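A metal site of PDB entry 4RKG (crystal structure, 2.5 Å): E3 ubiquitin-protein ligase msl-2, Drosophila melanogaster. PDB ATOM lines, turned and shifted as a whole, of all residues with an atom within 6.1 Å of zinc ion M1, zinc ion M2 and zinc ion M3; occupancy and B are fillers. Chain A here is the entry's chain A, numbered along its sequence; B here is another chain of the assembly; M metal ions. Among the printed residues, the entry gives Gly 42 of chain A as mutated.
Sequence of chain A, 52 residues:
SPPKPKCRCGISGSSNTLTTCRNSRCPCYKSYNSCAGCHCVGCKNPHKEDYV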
ATOM      1  N   LYS A   6      16.082  -6.658   7.932  1.00  0.00           N
ATOM      2  CA  LYS A   6      14.672  -6.473   8.355  1.00  0.00           C
ATOM      3  C   LYS A   6      13.898  -7.804   8.490  1.00  0.00           C
ATOM      4  O   LYS A   6      13.375  -8.308   7.497  1.00  0.00           O
ATOM      5  CB  LYS A   6      13.932  -5.574   7.350  1.00  0.00           C
ATOM      6  CG  LYS A   6      13.797  -4.101   7.753  1.00  0.00           C
ATOM      7  CD  LYS A   6      13.289  -3.249   6.589  1.00  0.00           C
ATOM      8  CE  LYS A   6      14.447  -2.684   5.761  1.00  0.00           C
ATOM      9  NZ  LYS A   6      15.338  -1.792   6.566  1.00  0.00           N
ATOM     10  N   CYS A   7      13.801  -8.346   9.714  1.00  0.00           N
ATOM     11  CA  CYS A   7      13.256  -9.702   9.934  1.00  0.00           C
ATOM     12  C   CYS A   7      11.724  -9.775   9.933  1.00  0.00           C
ATOM     13  O   CYS A   7      11.025  -8.763   9.745  1.00  0.00           O
ATOM     14  CB  CYS A   7      13.801 -10.328  11.235  1.00  0.00           C
ATOM     15  SG  CYS A   7      13.430  -9.569  12.843  1.00  0.00           S
ATOM     16  N   ARG A   8      11.215 -10.988  10.101  1.00  0.00           N
ATOM     17  CA  ARG A   8       9.790 -11.235  10.127  1.00  0.00           C
ATOM     18  C   ARG A   8       9.466 -12.406  11.073  1.00  0.00           C
ATOM     19  O   ARG A   8       8.586 -13.233  10.784  1.00  0.00           O
ATOM     20  CB  ARG A   8       9.272 -11.494   8.698  1.00  0.00           C
ATOM     21  CG  ARG A   8       8.790 -10.224   8.008  1.00  0.00           C
ATOM     22  CD  ARG A   8       8.463 -10.468   6.525  1.00  0.00           C
ATOM     23  NE  ARG A   8       7.405 -11.452   6.343  1.00  0.00           N
ATOM     24  CZ  ARG A   8       7.473 -12.491   5.515  1.00  0.00           C
ATOM     25  NH1 ARG A   8       6.456 -13.348   5.433  1.00  0.00           N
ATOM     26  NH2 ARG A   8       8.561 -12.679   4.781  1.00  0.00           N
ATOM     27  N   CYS A   9      10.182 -12.459  12.192  1.00  0.00           N
ATOM     28  CA  CYS A   9       9.950 -13.433  13.264  1.00  0.00           C
ATOM     29  C   CYS A   9       8.658 -13.135  14.022  1.00  0.00           C
ATOM     30  O   CYS A   9       8.421 -12.007  14.399  1.00  0.00           O
ATOM     31  CB  CYS A   9      11.116 -13.443  14.262  1.00  0.00           C
ATOM     32  SG  CYS A   9      12.784 -13.324  13.553  1.00  0.00           S
ATOM     33  N   THR A  20      11.765 -15.152  20.541  1.00  0.00           N
ATOM     34  CA  THR A  20      11.532 -14.449  19.282  1.00  0.00           C
ATOM     35  C   THR A  20      12.495 -13.288  19.102  1.00  0.00           C
ATOM     36  O   THR A  20      12.559 -12.369  19.928  1.00  0.00           O
ATOM     37  CB  THR A  20      10.103 -13.885  19.177  1.00  0.00           C
ATOM     38  OG1 THR A  20       9.179 -14.958  18.965  1.00  0.00           O
ATOM     39  CG2 THR A  20      10.010 -12.926  18.012  1.00  0.00           C
ATOM     40  N   CYS A  21      13.273 -13.350  18.021  1.00  0.00           N
ATOM     41  CA  CYS A  21      14.365 -12.419  17.753  1.00  0.00           C
ATOM     42  C   CYS A  21      15.393 -12.465  18.881  1.00  0.00           C
ATOM     43  O   CYS A  21      16.150 -11.518  19.088  1.00  0.00           O
ATOM     44  CB  CYS A  21      13.854 -10.985  17.576  1.00  0.00           C
ATOM     45  SG  CYS A  21      12.688 -10.745  16.221  1.00  0.00           S
ATOM     46  N   ARG A  22      15.417 -13.568  19.617  1.00  0.00           N
ATOM     47  CA  ARG A  22      16.438 -13.756  20.641  1.00  0.00           C
ATOM     48  C   ARG A  22      17.211 -15.041  20.347  1.00  0.00           C
ATOM     49  O   ARG A  22      17.566 -15.761  21.263  1.00  0.00           O
ATOM     50  CB  ARG A  22      15.825 -13.800  22.039  1.00  0.00           C
ATOM     51  CG  ARG A  22      16.819 -13.499  23.146  1.00  0.00           C
ATOM     52  CD  ARG A  22      16.311 -13.894  24.500  1.00  0.00           C
ATOM     53  NE  ARG A  22      17.158 -13.326  25.543  1.00  0.00           N
ATOM     54  CZ  ARG A  22      16.995 -12.117  26.045  1.00  0.00           C
ATOM     55  NH1 ARG A  22      16.009 -11.340  25.617  1.00  0.00           N
ATOM     56  NH2 ARG A  22      17.814 -11.675  26.994  1.00  0.00           N
ATOM     57  N   CYS A  26      17.052 -15.700  13.886  1.00  0.00           N
ATOM     58  CA  CYS A  26      16.779 -14.306  13.552  1.00  0.00           C
ATOM     59  C   CYS A  26      18.065 -13.630  13.087  1.00  0.00           C
ATOM     60  O   CYS A  26      19.072 -13.713  13.779  1.00  0.00           O
ATOM     61  CB  CYS A  26      16.170 -13.558  14.758  1.00  0.00           C
ATOM     62  SG  CYS A  26      16.111 -11.733  14.640  1.00  0.00           S
ATOM     63  N   PRO A  27      18.032 -12.994  11.917  1.00  0.00           N
ATOM     64  CA  PRO A  27      19.174 -12.297  11.307  1.00  0.00           C
ATOM     65  C   PRO A  27      19.783 -11.213  12.164  1.00  0.00           C
ATOM     66  O   PRO A  27      20.974 -11.262  12.468  1.00  0.00           O
ATOM     67  CB  PRO A  27      18.575 -11.673  10.036  1.00  0.00           C
ATOM     68  CG  PRO A  27      17.107 -11.896  10.115  1.00  0.00           C
ATOM     69  CD  PRO A  27      16.910 -13.087  10.981  1.00  0.00           C
ATOM     70  N   CYS A  28      18.965 -10.239  12.534  1.00  0.00           N
ATOM     71  CA  CYS A  28      19.407  -9.096  13.331  1.00  0.00           C
ATOM     72  C   CYS A  28      20.100  -9.527  14.627  1.00  0.00           C
ATOM     73  O   CYS A  28      21.170  -9.012  14.965  1.00  0.00           O
ATOM     74  CB  CYS A  28      18.199  -8.210  13.644  1.00  0.00           C
ATOM     75  SG  CYS A  28      16.813  -8.440  12.485  1.00  0.00           S
ATOM     76  N   TYR A  29      19.490 -10.472  15.333  1.00  0.00           N
ATOM     77  CA  TYR A  29      20.102 -11.071  16.505  1.00  0.00           C
ATOM     78  C   TYR A  29      21.482 -11.612  16.139  1.00  0.00           C
ATOM     79  O   TYR A  29      22.490 -11.189  16.688  1.00  0.00           O
ATOM     80  CB  TYR A  29      19.234 -12.204  17.068  1.00  0.00           C
ATOM     81  CG  TYR A  29      19.489 -12.549  18.515  1.00  0.00           C
ATOM     82  CD1 TYR A  29      19.099 -11.687  19.540  1.00  0.00           C
ATOM     83  CD2 TYR A  29      20.108 -13.733  18.873  1.00  0.00           C
ATOM     84  CE1 TYR A  29      19.313 -11.997  20.869  1.00  0.00           C
ATOM     85  CE2 TYR A  29      20.335 -14.055  20.211  1.00  0.00           C
ATOM     86  CZ  TYR A  29      19.928 -13.185  21.204  1.00  0.00           C
ATOM     87  OH  TYR A  29      20.142 -13.495  22.533  1.00  0.00           O
ATOM     88  N   ASN A  33      22.507  -7.026  15.545  1.00  0.00           N
ATOM     89  CA  ASN A  33      21.819  -5.752  15.374  1.00  0.00           C
ATOM     90  C   ASN A  33      20.419  -5.797  15.956  1.00  0.00           C
ATOM     91  O   ASN A  33      19.892  -6.877  16.229  1.00  0.00           O
ATOM     92  CB  ASN A  33      21.752  -5.367  13.891  1.00  0.00           C
ATOM     93  CG  ASN A  33      23.099  -5.407  13.240  1.00  0.00           C
ATOM     94  OD1 ASN A  33      23.436  -6.373  12.558  1.00  0.00           O
ATOM     95  ND2 ASN A  33      23.901  -4.355  13.463  1.00  0.00           N
ATOM     96  N   SER A  34      19.824  -4.625  16.167  1.00  0.00           N
ATOM     97  CA  SER A  34      18.481  -4.515  16.729  1.00  0.00           C
ATOM     98  C   SER A  34      17.413  -4.752  15.664  1.00  0.00           C
ATOM     99  O   SER A  34      17.737  -5.001  14.499  1.00  0.00           O
ATOM    100  CB  SER A  34      18.276  -3.132  17.360  1.00  0.00           C
ATOM    101  OG  SER A  34      18.297  -2.120  16.357  1.00  0.00           O
ATOM    102  N   CYS A  35      16.153  -4.680  16.047  1.00  0.00           N
ATOM    103  CA  CYS A  35      15.071  -4.850  15.077  1.00  0.00           C
ATOM    104  C   CYS A  35      14.466  -3.508  14.720  1.00  0.00           C
ATOM    105  O   CYS A  35      13.250  -3.357  14.624  1.00  0.00           O
ATOM    106  CB  CYS A  35      14.012  -5.806  15.603  1.00  0.00           C
ATOM    107  SG  CYS A  35      14.549  -7.489  15.587  1.00  0.00           S
ATOM    108  N   ALA A  36      15.328  -2.514  14.541  1.00  0.00           N
ATOM    109  CA  ALA A  36      14.912  -1.215  14.050  1.00  0.00           C
ATOM    110  C   ALA A  36      14.341  -1.356  12.641  1.00  0.00           C
ATOM    111  O   ALA A  36      15.068  -1.714  11.710  1.00  0.00           O
ATOM    112  CB  ALA A  36      16.097  -0.245  14.072  1.00  0.00           C
ATOM    113  N   CYS A  38      12.171  -3.523  11.604  1.00  0.00           N
ATOM    114  CA  CYS A  38      11.742  -4.894  11.330  1.00  0.00           C
ATOM    115  C   CYS A  38      10.216  -5.067  11.337  1.00  0.00           C
ATOM    116  O   CYS A  38       9.487  -4.168  11.721  1.00  0.00           O
ATOM    117  CB  CYS A  38      12.360  -5.866  12.343  1.00  0.00           C
ATOM    118  SG  CYS A  38      14.119  -6.319  12.119  1.00  0.00           S
ATOM    119  N   HIS A  39       9.752  -6.232  10.931  1.00  0.00           N
ATOM    120  CA  HIS A  39       8.314  -6.501  10.875  1.00  0.00           C
ATOM    121  C   HIS A  39       7.914  -7.666  11.781  1.00  0.00           C
ATOM    122  O   HIS A  39       6.798  -8.169  11.714  1.00  0.00           O
ATOM    123  CB  HIS A  39       7.921  -6.749   9.416  1.00  0.00           C
ATOM    124  CG  HIS A  39       7.878  -5.499   8.623  1.00  0.00           C
ATOM    125  ND1 HIS A  39       8.215  -5.441   7.286  1.00  0.00           N
ATOM    126  CD2 HIS A  39       7.577  -4.223   8.987  1.00  0.00           C
ATOM    127  CE1 HIS A  39       8.095  -4.190   6.862  1.00  0.00           C
ATOM    128  NE2 HIS A  39       7.713  -3.437   7.877  1.00  0.00           N
ATOM    129  N   CYS A  40       8.851  -8.068  12.619  1.00  0.00           N
ATOM    130  CA  CYS A  40       8.642  -9.035  13.690  1.00  0.00           C
ATOM    131  C   CYS A  40       7.463  -8.699  14.612  1.00  0.00           C
ATOM    132  O   CYS A  40       6.971  -7.570  14.655  1.00  0.00           O
ATOM    133  CB  CYS A  40       9.930  -9.155  14.508  1.00  0.00           C
ATOM    134  SG  CYS A  40      10.724  -7.543  14.890  1.00  0.00           S
ATOM    135  N   VAL A  41       7.011  -9.692  15.361  1.00  0.00           N
ATOM    136  CA  VAL A  41       5.881  -9.551  16.273  1.00  0.00           C
ATOM    137  C   VAL A  41       6.287 -10.198  17.588  1.00  0.00           C
ATOM    138  O   VAL A  41       6.847 -11.288  17.594  1.00  0.00           O
ATOM    139  CB  VAL A  41       4.605 -10.225  15.712  1.00  0.00           C
ATOM    140  CG1 VAL A  41       3.453 -10.082  16.636  1.00  0.00           C
ATOM    141  CG2 VAL A  41       4.246  -9.653  14.332  1.00  0.00           C
ATOM    142  N   GLY A  42       6.035  -9.521  18.692  1.00  0.00           N
ATOM    143  CA  GLY A  42       6.439 -10.043  19.984  1.00  0.00           C
ATOM    144  C   GLY A  42       7.954 -10.183  20.002  1.00  0.00           C
ATOM    145  O   GLY A  42       8.486 -11.190  20.467  1.00  0.00           O
ATOM    146  N   CYS A  43       8.621  -9.169  19.471  1.00  0.00           N
ATOM    147  CA  CYS A  43      10.081  -9.113  19.462  1.00  0.00           C
ATOM    148  C   CYS A  43      10.638  -9.131  20.868  1.00  0.00           C
ATOM    149  O   CYS A  43      10.134  -8.441  21.741  1.00  0.00           O
ATOM    150  CB  CYS A  43      10.568  -7.865  18.732  1.00  0.00           C
ATOM    151  SG  CYS A  43      12.393  -7.856  18.552  1.00  0.00           S
ATOM    152  N   LYS A  44      11.678  -9.916  21.087  1.00  0.00           N
ATOM    153  CA  LYS A  44      12.323  -9.967  22.385  1.00  0.00           C
ATOM    154  C   LYS A  44      13.811  -9.790  22.165  1.00  0.00           C
ATOM    155  O   LYS A  44      14.628 -10.183  22.985  1.00  0.00           O
ATOM    156  CB  LYS A  44      12.015 -11.279  23.102  1.00  0.00           C
ATOM    157  CG  LYS A  44      10.532 -11.618  23.218  1.00  0.00           C
ATOM    158  CD  LYS A  44      10.028 -11.437  24.621  1.00  0.00           C
ATOM    159  CE  LYS A  44       9.010 -12.505  25.040  1.00  0.00           C
ATOM    160  NZ  LYS A  44       7.900 -12.694  24.082  1.00  0.00           N
ATOM    161  N   ASN A  45      14.157  -9.199  21.036  1.00  0.00           N
ATOM    162  CA  ASN A  45      15.522  -8.804  20.761  1.00  0.00           C
ATOM    163  C   ASN A  45      15.997  -7.780  21.775  1.00  0.00           C
ATOM    164  O   ASN A  45      15.484  -6.669  21.800  1.00  0.00           O
ATOM    165  CB  ASN A  45      15.633  -8.229  19.357  1.00  0.00           C
ATOM    166  CG  ASN A  45      17.059  -8.090  18.897  1.00  0.00           C
ATOM    167  OD1 ASN A  45      17.981  -8.001  19.709  1.00  0.00           O
ATOM    168  ND2 ASN A  45      17.264  -8.087  17.583  1.00  0.00           N
ATOM    169  P    DG B   5      10.663 -17.300  13.477  1.00  0.00           P
ATOM    170  OP1  DG B   5      11.434 -17.182  14.741  1.00  0.00           O
ATOM    171  OP2  DG B   5       9.249 -16.875  13.404  1.00  0.00           O
ATOM    172  O5'  DG B   5      11.481 -16.562  12.322  1.00  0.00           O
ATOM    173  C5'  DG B   5      12.842 -16.874  12.156  1.00  0.00           C
ATOM    174  C4'  DG B   5      13.295 -16.665  10.728  1.00  0.00           C
ATOM    175  O4'  DG B   5      12.788 -17.730   9.886  1.00  0.00           O
ATOM    176  C3'  DG B   5      12.816 -15.391  10.062  1.00  0.00           C
ATOM    177  O3'  DG B   5      13.777 -15.054   9.106  1.00  0.00           O
ATOM    178  C2'  DG B   5      11.501 -15.829   9.417  1.00  0.00           C
ATOM    179  C1'  DG B   5      11.876 -17.218   8.940  1.00  0.00           C
ATOM    180  N9   DG B   5      10.763 -18.129   8.922  1.00  0.00           N
ATOM    181  C8   DG B   5       9.795 -18.278   9.887  1.00  0.00           C
ATOM    182  N7   DG B   5       8.947 -19.229   9.624  1.00  0.00           N
ATOM    183  C5   DG B   5       9.409 -19.768   8.431  1.00  0.00           C
ATOM    184  C6   DG B   5       8.894 -20.829   7.653  1.00  0.00           C
ATOM    185  O6   DG B   5       7.894 -21.527   7.892  1.00  0.00           O
ATOM    186  N1   DG B   5       9.655 -21.046   6.510  1.00  0.00           N
ATOM    187  C2   DG B   5      10.761 -20.317   6.160  1.00  0.00           C
ATOM    188  N2   DG B   5      11.360 -20.674   5.005  1.00  0.00           N
ATOM    189  N3   DG B   5      11.253 -19.326   6.871  1.00  0.00           N
ATOM    190  C4   DG B   5      10.524 -19.105   7.995  1.00  0.00           C
ATOM    191  P    DC B   6      13.588 -13.762   8.197  1.00  0.00           P
ATOM    192  OP1  DC B   6      14.967 -13.252   8.000  1.00  0.00           O
ATOM    193  OP2  DC B   6      12.526 -12.890   8.735  1.00  0.00           O
ATOM    194  O5'  DC B   6      13.080 -14.370   6.822  1.00  0.00           O
ATOM    195  C5'  DC B   6      13.890 -15.287   6.132  1.00  0.00           C
ATOM    196  C4'  DC B   6      13.223 -15.695   4.846  1.00  0.00           C
ATOM    197  O4'  DC B   6      12.086 -16.547   5.156  1.00  0.00           O
ATOM    198  C3'  DC B   6      12.670 -14.540   4.003  1.00  0.00           C
ATOM    199  O3'  DC B   6      12.781 -14.885   2.646  1.00  0.00           O
ATOM    200  C2'  DC B   6      11.200 -14.520   4.437  1.00  0.00           C
ATOM    201  C1'  DC B   6      10.951 -16.014   4.502  1.00  0.00           C
ATOM    202  N1   DC B   6       9.736 -16.421   5.251  1.00  0.00           N
ATOM    203  C2   DC B   6       9.037 -17.550   4.833  1.00  0.00           C
ATOM    204  O2   DC B   6       9.456 -18.172   3.860  1.00  0.00           O
ATOM    205  N3   DC B   6       7.944 -17.947   5.507  1.00  0.00           N
ATOM    206  C4   DC B   6       7.541 -17.243   6.575  1.00  0.00           C
ATOM    207  N4   DC B   6       6.443 -17.668   7.217  1.00  0.00           N
ATOM    208  C5   DC B   6       8.233 -16.075   7.017  1.00  0.00           C
ATOM    209  C6   DC B   6       9.324 -15.700   6.335  1.00  0.00           C
HETATM  210 ZN    ZN M   1      13.839 -11.330  14.239  1.00  0.00          ZN
HETATM  211 ZN    ZN M   2      12.536  -8.536  16.407  1.00  0.00          ZN
HETATM  212 ZN    ZN M   3      14.666  -7.996  13.411  1.00  0.00          ZN
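The side-chain sulfur of Cys 26 lies close to the backbone NH of Tyr 29, 3.7 Å away.
The side-chain sulfur (SG) of Cys 43 lies close to the backbone NH (N) of Asn 45 (3.3 Å).
The backbone carbonyl oxygen of Cys 7 sits at hydrogen-bond distance from the backbone NH of His 39 (3.1 Å).
The side-chain sulfur of Cys 9 sits close to O5' of DG 5 of chain B.
The side-chain sulfur (SG) of Cys 35 sits close to the side-chain amide nitrogen (ND2) of Asn 45 (3.4 Å).
N of Asn 33 sits at hydrogen-bond distance from O of Cys 28.
N of Val 41 is in hydrogen-bond range of O of Cys 9 (2.9 Å).
Within 4 Å of zinc ion M1: Cys 7, Cys 9, Cys 21 and Cys 26.
Within 4 Å of zinc ion M2: Cys 7, Cys 21, Cys 35, Cys 40 and Cys 43.
The nearest printed residue that does not touch zinc ion M2 is Asn 45 (4.3 Å).
Of the 25 residues printed, 4 come within 4 Å of zinc ion M3.
Along chain A the residues within 4 Å of zinc ion M3 span positions 7 to 38.
The nearest printed residue that does not touch zinc ion M3 is Cys 26 (4.2 Å).
Zinc ion M1 is bound by the side-chain sulfur (SG) of Cys 7 (2.3 Å), the side-chain sulfur (SG) of Cys 26 (2.3 Å), the side-chain sulfur (SG) of Cys 9 (2.4 Å) and the side-chain sulfur (SG) of Cys 21 (2.4 Å).
Zinc ion M1 has four donor atoms within binding distance.
Zinc ion M2 is bound by the side-chain sulfur of Cys 21 (2.2 Å), the side-chain sulfur of Cys 43 (2.3 Å), the side-chain sulfur of Cys 35 (2.4 Å) and the side-chain sulfur of Cys 40 (2.6 Å).
Zinc ion M3 is bound by SG of Cys 7 (2.1 Å), SG of Cys 38 (2.2 Å), SG of Cys 35 (2.2 Å) and SG of Cys 28 (2.4 Å).
Zinc ion M3 has four donor atoms within binding distance.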
